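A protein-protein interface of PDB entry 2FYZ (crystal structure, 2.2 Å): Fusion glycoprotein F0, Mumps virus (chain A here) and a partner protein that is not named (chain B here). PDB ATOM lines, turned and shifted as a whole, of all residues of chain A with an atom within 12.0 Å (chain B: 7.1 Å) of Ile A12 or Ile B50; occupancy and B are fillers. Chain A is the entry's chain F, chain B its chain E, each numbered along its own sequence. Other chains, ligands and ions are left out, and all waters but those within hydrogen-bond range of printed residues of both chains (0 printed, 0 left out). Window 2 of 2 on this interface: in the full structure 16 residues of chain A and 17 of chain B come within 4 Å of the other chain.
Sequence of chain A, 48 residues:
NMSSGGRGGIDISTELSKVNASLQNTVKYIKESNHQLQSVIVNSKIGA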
ATOM      1  N   ARG A   7     -11.155   5.337 -25.610  1.00  0.00           N
ATOM      2  CA  ARG A   7     -12.179   4.348 -25.152  1.00  0.00           C
ATOM      3  C   ARG A   7     -13.597   4.919 -25.278  1.00  0.00           C
ATOM      4  O   ARG A   7     -13.836   6.113 -25.076  1.00  0.00           O
ATOM      5  CB  ARG A   7     -11.924   3.926 -23.692  1.00  0.00           C
ATOM      6  CG  ARG A   7     -13.129   4.155 -22.741  1.00  0.00           C
ATOM      7  CD  ARG A   7     -12.873   3.556 -21.370  1.00  0.00           C
ATOM      8  NE  ARG A   7     -14.056   3.622 -20.509  1.00  0.00           N
ATOM      9  CZ  ARG A   7     -14.197   2.943 -19.376  1.00  0.00           C
ATOM     10  NH1 ARG A   7     -13.226   2.137 -18.956  1.00  0.00           N
ATOM     11  NH2 ARG A   7     -15.318   3.049 -18.677  1.00  0.00           N
ATOM     12  N   GLY A   8     -14.537   4.049 -25.622  1.00  0.00           N
ATOM     13  CA  GLY A   8     -15.915   4.469 -25.764  1.00  0.00           C
ATOM     14  C   GLY A   8     -16.450   4.995 -24.446  1.00  0.00           C
ATOM     15  O   GLY A   8     -17.169   6.010 -24.416  1.00  0.00           O
ATOM     16  N   GLY A   9     -16.111   4.314 -23.352  1.00  0.00           N
ATOM     17  CA  GLY A   9     -16.590   4.749 -22.051  1.00  0.00           C
ATOM     18  C   GLY A   9     -16.235   6.200 -21.763  1.00  0.00           C
ATOM     19  O   GLY A   9     -17.091   6.986 -21.355  1.00  0.00           O
ATOM     20  N   ILE A  10     -14.975   6.573 -21.976  1.00  0.00           N
ATOM     21  CA  ILE A  10     -14.532   7.942 -21.721  1.00  0.00           C
ATOM     22  C   ILE A  10     -15.271   8.939 -22.611  1.00  0.00           C
ATOM     23  O   ILE A  10     -15.779   9.951 -22.131  1.00  0.00           O
ATOM     24  CB  ILE A  10     -13.008   8.085 -21.962  1.00  0.00           C
ATOM     25  CG1 ILE A  10     -12.244   7.382 -20.827  1.00  0.00           C
ATOM     26  CG2 ILE A  10     -12.610   9.563 -22.027  1.00  0.00           C
ATOM     27  CD1 ILE A  10     -10.773   7.140 -21.107  1.00  0.00           C
ATOM     28  N   ASP A  11     -15.328   8.655 -23.905  1.00  0.00           N
ATOM     29  CA  ASP A  11     -15.972   9.563 -24.825  1.00  0.00           C
ATOM     30  C   ASP A  11     -17.445   9.766 -24.554  1.00  0.00           C
ATOM     31  O   ASP A  11     -17.944  10.882 -24.693  1.00  0.00           O
ATOM     32  CB  ASP A  11     -15.760   9.088 -26.251  1.00  0.00           C
ATOM     33  CG  ASP A  11     -14.333   9.231 -26.685  1.00  0.00           C
ATOM     34  OD1 ASP A  11     -13.585   9.940 -25.979  1.00  0.00           O
ATOM     35  OD2 ASP A  11     -13.965   8.649 -27.729  1.00  0.00           O
ATOM     36  N   ILE A  12     -18.148   8.697 -24.190  1.00  0.00           N
ATOM     37  CA  ILE A  12     -19.558   8.831 -23.872  1.00  0.00           C
ATOM     38  C   ILE A  12     -19.650   9.683 -22.607  1.00  0.00           C
ATOM     39  O   ILE A  12     -20.529  10.539 -22.485  1.00  0.00           O
ATOM     40  CB  ILE A  12     -20.194   7.456 -23.634  1.00  0.00           C
ATOM     41  CG1 ILE A  12     -20.376   6.752 -24.981  1.00  0.00           C
ATOM     42  CG2 ILE A  12     -21.519   7.591 -22.907  1.00  0.00           C
ATOM     43  CD1 ILE A  12     -20.855   5.323 -24.861  1.00  0.00           C
ATOM     44  N   SER A  13     -18.732   9.461 -21.668  1.00  0.00           N
ATOM     45  CA  SER A  13     -18.735  10.230 -20.431  1.00  0.00           C
ATOM     46  C   SER A  13     -18.516  11.704 -20.751  1.00  0.00           C
ATOM     47  O   SER A  13     -19.119  12.588 -20.139  1.00  0.00           O
ATOM     48  CB  SER A  13     -17.638   9.739 -19.480  1.00  0.00           C
ATOM     49  OG  SER A  13     -17.544  10.587 -18.344  1.00  0.00           O
ATOM     50  N   THR A  14     -17.647  11.962 -21.720  1.00  0.00           N
ATOM     51  CA  THR A  14     -17.354  13.333 -22.128  1.00  0.00           C
ATOM     52  C   THR A  14     -18.577  13.943 -22.793  1.00  0.00           C
ATOM     53  O   THR A  14     -18.915  15.104 -22.553  1.00  0.00           O
ATOM     54  CB  THR A  14     -16.159  13.380 -23.100  1.00  0.00           C
ATOM     55  OG1 THR A  14     -14.971  13.030 -22.389  1.00  0.00           O
ATOM     56  CG2 THR A  14     -15.996  14.780 -23.698  1.00  0.00           C
ATOM     57  N   GLU A  15     -19.242  13.152 -23.626  1.00  0.00           N
ATOM     58  CA  GLU A  15     -20.442  13.611 -24.309  1.00  0.00           C
ATOM     59  C   GLU A  15     -21.506  13.997 -23.268  1.00  0.00           C
ATOM     60  O   GLU A  15     -22.135  15.051 -23.367  1.00  0.00           O
ATOM     61  CB  GLU A  15     -20.962  12.501 -25.221  1.00  0.00           C
ATOM     62  CG  GLU A  15     -21.981  12.953 -26.256  1.00  0.00           C
ATOM     63  CD  GLU A  15     -21.412  13.966 -27.236  1.00  0.00           C
ATOM     64  OE1 GLU A  15     -20.180  13.963 -27.457  1.00  0.00           O
ATOM     65  OE2 GLU A  15     -22.198  14.757 -27.802  1.00  0.00           O
ATOM     66  N   LEU A  16     -21.697  13.144 -22.266  1.00  0.00           N
ATOM     67  CA  LEU A  16     -22.671  13.416 -21.213  1.00  0.00           C
ATOM     68  C   LEU A  16     -22.309  14.655 -20.397  1.00  0.00           C
ATOM     69  O   LEU A  16     -23.187  15.347 -19.901  1.00  0.00           O
ATOM     70  CB  LEU A  16     -22.816  12.201 -20.296  1.00  0.00           C
ATOM     71  CG  LEU A  16     -23.846  11.172 -20.778  1.00  0.00           C
ATOM     72  CD1 LEU A  16     -25.243  11.681 -20.513  1.00  0.00           C
ATOM     73  CD2 LEU A  16     -23.665  10.909 -22.262  1.00  0.00           C
ATOM     74  N   SER A  17     -21.018  14.931 -20.251  1.00  0.00           N
ATOM     75  CA  SER A  17     -20.596  16.123 -19.526  1.00  0.00           C
ATOM     76  C   SER A  17     -20.913  17.355 -20.379  1.00  0.00           C
ATOM     77  O   SER A  17     -21.201  18.428 -19.850  1.00  0.00           O
ATOM     78  CB  SER A  17     -19.094  16.069 -19.220  1.00  0.00           C
ATOM     79  OG  SER A  17     -18.805  15.061 -18.267  1.00  0.00           O
ATOM     80  N   LYS A  18     -20.838  17.209 -21.699  1.00  0.00           N
ATOM     81  CA  LYS A  18     -21.158  18.321 -22.589  1.00  0.00           C
ATOM     82  C   LYS A  18     -22.638  18.634 -22.358  1.00  0.00           C
ATOM     83  O   LYS A  18     -23.033  19.789 -22.234  1.00  0.00           O
ATOM     84  CB  LYS A  18     -20.971  17.925 -24.061  1.00  0.00           C
ATOM     85  CG  LYS A  18     -19.573  17.493 -24.480  1.00  0.00           C
ATOM     86  CD  LYS A  18     -18.707  18.680 -24.819  1.00  0.00           C
ATOM     87  CE  LYS A  18     -17.401  18.255 -25.480  1.00  0.00           C
ATOM     88  NZ  LYS A  18     -17.601  17.643 -26.821  1.00  0.00           N
ATOM     89  N   VAL A  19     -23.449  17.580 -22.313  1.00  0.00           N
ATOM     90  CA  VAL A  19     -24.890  17.712 -22.109  1.00  0.00           C
ATOM     91  C   VAL A  19     -25.192  18.520 -20.856  1.00  0.00           C
ATOM     92  O   VAL A  19     -25.937  19.505 -20.892  1.00  0.00           O
ATOM     93  CB  VAL A  19     -25.566  16.318 -21.949  1.00  0.00           C
ATOM     94  CG1 VAL A  19     -27.021  16.481 -21.520  1.00  0.00           C
ATOM     95  CG2 VAL A  19     -25.479  15.543 -23.254  1.00  0.00           C
ATOM     96  N   ASN A  20     -24.606  18.081 -19.749  1.00  0.00           N
ATOM     97  CA  ASN A  20     -24.807  18.722 -18.459  1.00  0.00           C
ATOM     98  C   ASN A  20     -24.374  20.188 -18.452  1.00  0.00           C
ATOM     99  O   ASN A  20     -25.001  21.025 -17.794  1.00  0.00           O
ATOM    100  CB  ASN A  20     -24.060  17.938 -17.376  1.00  0.00           C
ATOM    101  CG  ASN A  20     -24.185  18.578 -16.006  1.00  0.00           C
ATOM    102  OD1 ASN A  20     -23.485  19.539 -15.692  1.00  0.00           O
ATOM    103  ND2 ASN A  20     -25.096  18.058 -15.187  1.00  0.00           N
ATOM    104  N   ALA A  21     -23.307  20.499 -19.182  1.00  0.00           N
ATOM    105  CA  ALA A  21     -22.824  21.877 -19.247  1.00  0.00           C
ATOM    106  C   ALA A  21     -23.829  22.728 -20.017  1.00  0.00           C
ATOM    107  O   ALA A  21     -24.081  23.880 -19.665  1.00  0.00           O
ATOM    108  CB  ALA A  21     -21.465  21.931 -19.928  1.00  0.00           C
ATOM    109  N   LEU B  43     -26.917  14.637 -26.123  1.00  0.00           N
ATOM    110  CA  LEU B  43     -27.426  13.401 -25.560  1.00  0.00           C
ATOM    111  C   LEU B  43     -27.785  12.446 -26.697  1.00  0.00           C
ATOM    112  O   LEU B  43     -27.516  11.249 -26.620  1.00  0.00           O
ATOM    113  CB  LEU B  43     -28.649  13.688 -24.679  1.00  0.00           C
ATOM    114  CG  LEU B  43     -29.130  12.556 -23.768  1.00  0.00           C
ATOM    115  CD1 LEU B  43     -27.974  12.019 -22.930  1.00  0.00           C
ATOM    116  CD2 LEU B  43     -30.236  13.074 -22.867  1.00  0.00           C
ATOM    117  N   ALA B  44     -28.375  12.983 -27.761  1.00  0.00           N
ATOM    118  CA  ALA B  44     -28.761  12.165 -28.902  1.00  0.00           C
ATOM    119  C   ALA B  44     -27.518  11.537 -29.524  1.00  0.00           C
ATOM    120  O   ALA B  44     -27.515  10.360 -29.889  1.00  0.00           O
ATOM    121  CB  ALA B  44     -29.498  13.013 -29.924  1.00  0.00           C
ATOM    122  N   ILE B  45     -26.459  12.326 -29.641  1.00  0.00           N
ATOM    123  CA  ILE B  45     -25.215  11.827 -30.195  1.00  0.00           C
ATOM    124  C   ILE B  45     -24.677  10.707 -29.305  1.00  0.00           C
ATOM    125  O   ILE B  45     -24.188   9.691 -29.803  1.00  0.00           O
ATOM    126  CB  ILE B  45     -24.189  12.970 -30.324  1.00  0.00           C
ATOM    127  CG1 ILE B  45     -24.523  13.798 -31.565  1.00  0.00           C
ATOM    128  CG2 ILE B  45     -22.773  12.420 -30.423  1.00  0.00           C
ATOM    129  CD1 ILE B  45     -23.826  15.145 -31.609  1.00  0.00           C
ATOM    130  N   ALA B  46     -24.792  10.879 -27.990  1.00  0.00           N
ATOM    131  CA  ALA B  46     -24.324   9.873 -27.047  1.00  0.00           C
ATOM    132  C   ALA B  46     -25.160   8.609 -27.197  1.00  0.00           C
ATOM    133  O   ALA B  46     -24.640   7.491 -27.178  1.00  0.00           O
ATOM    134  CB  ALA B  46     -24.431  10.400 -25.626  1.00  0.00           C
ATOM    135  N   VAL B  47     -26.465   8.798 -27.341  1.00  0.00           N
ATOM    136  CA  VAL B  47     -27.385   7.685 -27.507  1.00  0.00           C
ATOM    137  C   VAL B  47     -27.104   6.930 -28.804  1.00  0.00           C
ATOM    138  O   VAL B  47     -27.193   5.700 -28.853  1.00  0.00           O
ATOM    139  CB  VAL B  47     -28.835   8.194 -27.487  1.00  0.00           C
ATOM    140  CG1 VAL B  47     -29.783   7.138 -28.025  1.00  0.00           C
ATOM    141  CG2 VAL B  47     -29.199   8.579 -26.061  1.00  0.00           C
ATOM    142  N   GLN B  48     -26.757   7.667 -29.852  1.00  0.00           N
ATOM    143  CA  GLN B  48     -26.450   7.057 -31.138  1.00  0.00           C
ATOM    144  C   GLN B  48     -25.178   6.220 -31.033  1.00  0.00           C
ATOM    145  O   GLN B  48     -25.041   5.197 -31.708  1.00  0.00           O
ATOM    146  CB  GLN B  48     -26.266   8.138 -32.204  1.00  0.00           C
ATOM    147  CG  GLN B  48     -25.679   7.632 -33.511  1.00  0.00           C
ATOM    148  CD  GLN B  48     -26.610   6.695 -34.245  1.00  0.00           C
ATOM    149  OE1 GLN B  48     -27.740   6.475 -33.827  1.00  0.00           O
ATOM    150  NE2 GLN B  48     -26.139   6.139 -35.354  1.00  0.00           N
ATOM    151  N   ALA B  49     -24.247   6.649 -30.185  1.00  0.00           N
ATOM    152  CA  ALA B  49     -22.999   5.910 -30.014  1.00  0.00           C
ATOM    153  C   ALA B  49     -23.235   4.633 -29.194  1.00  0.00           C
ATOM    154  O   ALA B  49     -22.597   3.604 -29.425  1.00  0.00           O
ATOM    155  CB  ALA B  49     -21.945   6.795 -29.345  1.00  0.00           C
ATOM    156  N   ILE B  50     -24.156   4.705 -28.240  1.00  0.00           N
ATOM    157  CA  ILE B  50     -24.483   3.552 -27.414  1.00  0.00           C
ATOM    158  C   ILE B  50     -25.220   2.529 -28.275  1.00  0.00           C
ATOM    159  O   ILE B  50     -25.133   1.321 -28.046  1.00  0.00           O
ATOM    160  CB  ILE B  50     -25.357   3.974 -26.216  1.00  0.00           C
ATOM    161  CG1 ILE B  50     -24.492   4.763 -25.226  1.00  0.00           C
ATOM    162  CG2 ILE B  50     -26.001   2.748 -25.564  1.00  0.00           C
ATOM    163  CD1 ILE B  50     -25.261   5.428 -24.102  1.00  0.00           C
ATOM    164  N   GLN B  51     -25.936   3.023 -29.279  1.00  0.00           N
ATOM    165  CA  GLN B  51     -26.666   2.158 -30.188  1.00  0.00           C
ATOM    166  C   GLN B  51     -25.681   1.394 -31.073  1.00  0.00           C
ATOM    167  O   GLN B  51     -25.779   0.176 -31.211  1.00  0.00           O
ATOM    168  CB  GLN B  51     -27.614   2.989 -31.061  1.00  0.00           C
ATOM    169  CG  GLN B  51     -28.352   2.204 -32.143  1.00  0.00           C
ATOM    170  CD  GLN B  51     -29.237   1.099 -31.584  1.00  0.00           C
ATOM    171  OE1 GLN B  51     -29.530   1.064 -30.390  1.00  0.00           O
ATOM    172  NE2 GLN B  51     -29.681   0.201 -32.456  1.00  0.00           N
ATOM    173  N   ASP B  52     -24.732   2.111 -31.670  1.00  0.00           N
ATOM    174  CA  ASP B  52     -23.743   1.478 -32.536  1.00  0.00           C
ATOM    175  C   ASP B  52     -23.021   0.370 -31.787  1.00  0.00           C
ATOM    176  O   ASP B  52     -22.804  -0.718 -32.318  1.00  0.00           O
ATOM    177  CB  ASP B  52     -22.707   2.495 -33.028  1.00  0.00           C
ATOM    178  CG  ASP B  52     -23.320   3.596 -33.872  1.00  0.00           C
ATOM    179  OD1 ASP B  52     -24.236   3.303 -34.667  1.00  0.00           O
ATOM    180  OD2 ASP B  52     -22.869   4.757 -33.751  1.00  0.00           O
ATOM    181  N   HIS B  53     -22.654   0.657 -30.545  1.00  0.00           N
ATOM    182  CA  HIS B  53     -21.948  -0.299 -29.706  1.00  0.00           C
ATOM    183  C   HIS B  53     -22.753  -1.579 -29.522  1.00  0.00           C
ATOM    184  O   HIS B  53     -22.235  -2.684 -29.679  1.00  0.00           O
ATOM    185  CB  HIS B  53     -21.661   0.334 -28.343  1.00  0.00           C
ATOM    186  CG  HIS B  53     -20.760  -0.478 -27.468  1.00  0.00           C
ATOM    187  ND1 HIS B  53     -20.401  -0.079 -26.199  1.00  0.00           N
ATOM    188  CD2 HIS B  53     -20.135  -1.663 -27.679  1.00  0.00           C
ATOM    189  CE1 HIS B  53     -19.597  -0.981 -25.665  1.00  0.00           C
ATOM    190  NE2 HIS B  53     -19.420  -1.952 -26.545  1.00  0.00           N
ATOM    191  N   ILE B  54     -24.028  -1.418 -29.188  1.00  0.00           N
ATOM    192  CA  ILE B  54     -24.918  -2.546 -28.962  1.00  0.00           C
ATOM    193  C   ILE B  54     -25.084  -3.443 -30.186  1.00  0.00           C
ATOM    194  O   ILE B  54     -25.226  -4.657 -30.054  1.00  0.00           O
ATOM    195  CB  ILE B  54     -26.303  -2.056 -28.508  1.00  0.00           C
ATOM    196  CG1 ILE B  54     -26.189  -1.422 -27.122  1.00  0.00           C
ATOM    197  CG2 ILE B  54     -27.298  -3.206 -28.502  1.00  0.00           C
ATOM    198  CD1 ILE B  54     -27.485  -0.841 -26.614  1.00  0.00           C
ATOM    199  N   ASN B  55     -25.065  -2.853 -31.375  1.00  0.00           N
ATOM    200  CA  ASN B  55     -25.226  -3.642 -32.585  1.00  0.00           C
ATOM    201  C   ASN B  55     -23.912  -4.029 -33.239  1.00  0.00           C
ATOM    202  O   ASN B  55     -23.899  -4.562 -34.349  1.00  0.00           O
ATOM    203  CB  ASN B  55     -26.103  -2.900 -33.590  1.00  0.00           C
ATOM    204  CG  ASN B  55     -27.552  -2.852 -33.164  1.00  0.00           C
ATOM    205  OD1 ASN B  55     -28.142  -3.878 -32.813  1.00  0.00           O
ATOM    206  ND2 ASN B  55     -28.139  -1.662 -33.199  1.00  0.00           N
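CG1 of Ile B50 touches CD1 of Ile A12, at 3.7 Å. Ile B45 touches Glu A15 (CG2 to OE2, 3.6 Å). Glu A15 touches Ala B46 (CG to CB, 3.6 Å). CD1 of Leu B43 touches CD1 of Leu A16, 3.7 Å away. CD2 of Leu A16 touches CB of Ala B46, at 3.5 Å. Val A19 touches Leu B43.
Printed residues of chain B within 4 Å of Glu A15: Ile B45 (3.6 Å) and Ala B46 (3.6 Å). Of the printed residues of chain B, Leu A16 touches Leu B43 (3.7 Å) and Ala B46 (3.5 Å). Printed residues of chain B within 4 Å of Val A19: Leu B43. Of the printed residues of chain A, Leu B43 touches Leu A16 and Val A19. Ala B46 touches just these residues of chain A: Glu A15 and Leu A16. Val B47 touches none of the printed residues of chain A. No residue of chain A comes within 4 Å of Gln B48. Of chain A, only Ile A12 comes within 4 Å of Ile B50. No residue of chain A comes within 4 Å of Gln B51. His B53 touches none of the printed residues of chain A. Ile B54 touches none of the printed residues of chain A. The nearest residue of chain B that does not touch Ile A12 is Ala B49 (4.6 Å). The nearest residue of chain A that does not touch Ile B50 is Leu A16 (6.0 Å).
Of the 15 printed residues of chain A, 4 touch a printed residue of chain B. Hydrophobic or aromatic side chains of chain A that line the printed part of chain B: Ile A12, Leu A16 and Val A19. Of the 13 printed residues of chain B, 4 touch a printed residue of chain A. Hydrophobic or aromatic side chains of chain B within 4 Å of the printed part of chain A: Leu B43, Ile B45, Ala B46 and Ile B50. Along chain B the printed residues that touch a printed residue of chain A span positions 43 to 50. Among the printed residues, no Asp or Glu carboxylate lies within 4 Å of a Lys or Arg side-chain nitrogen of the other chain.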
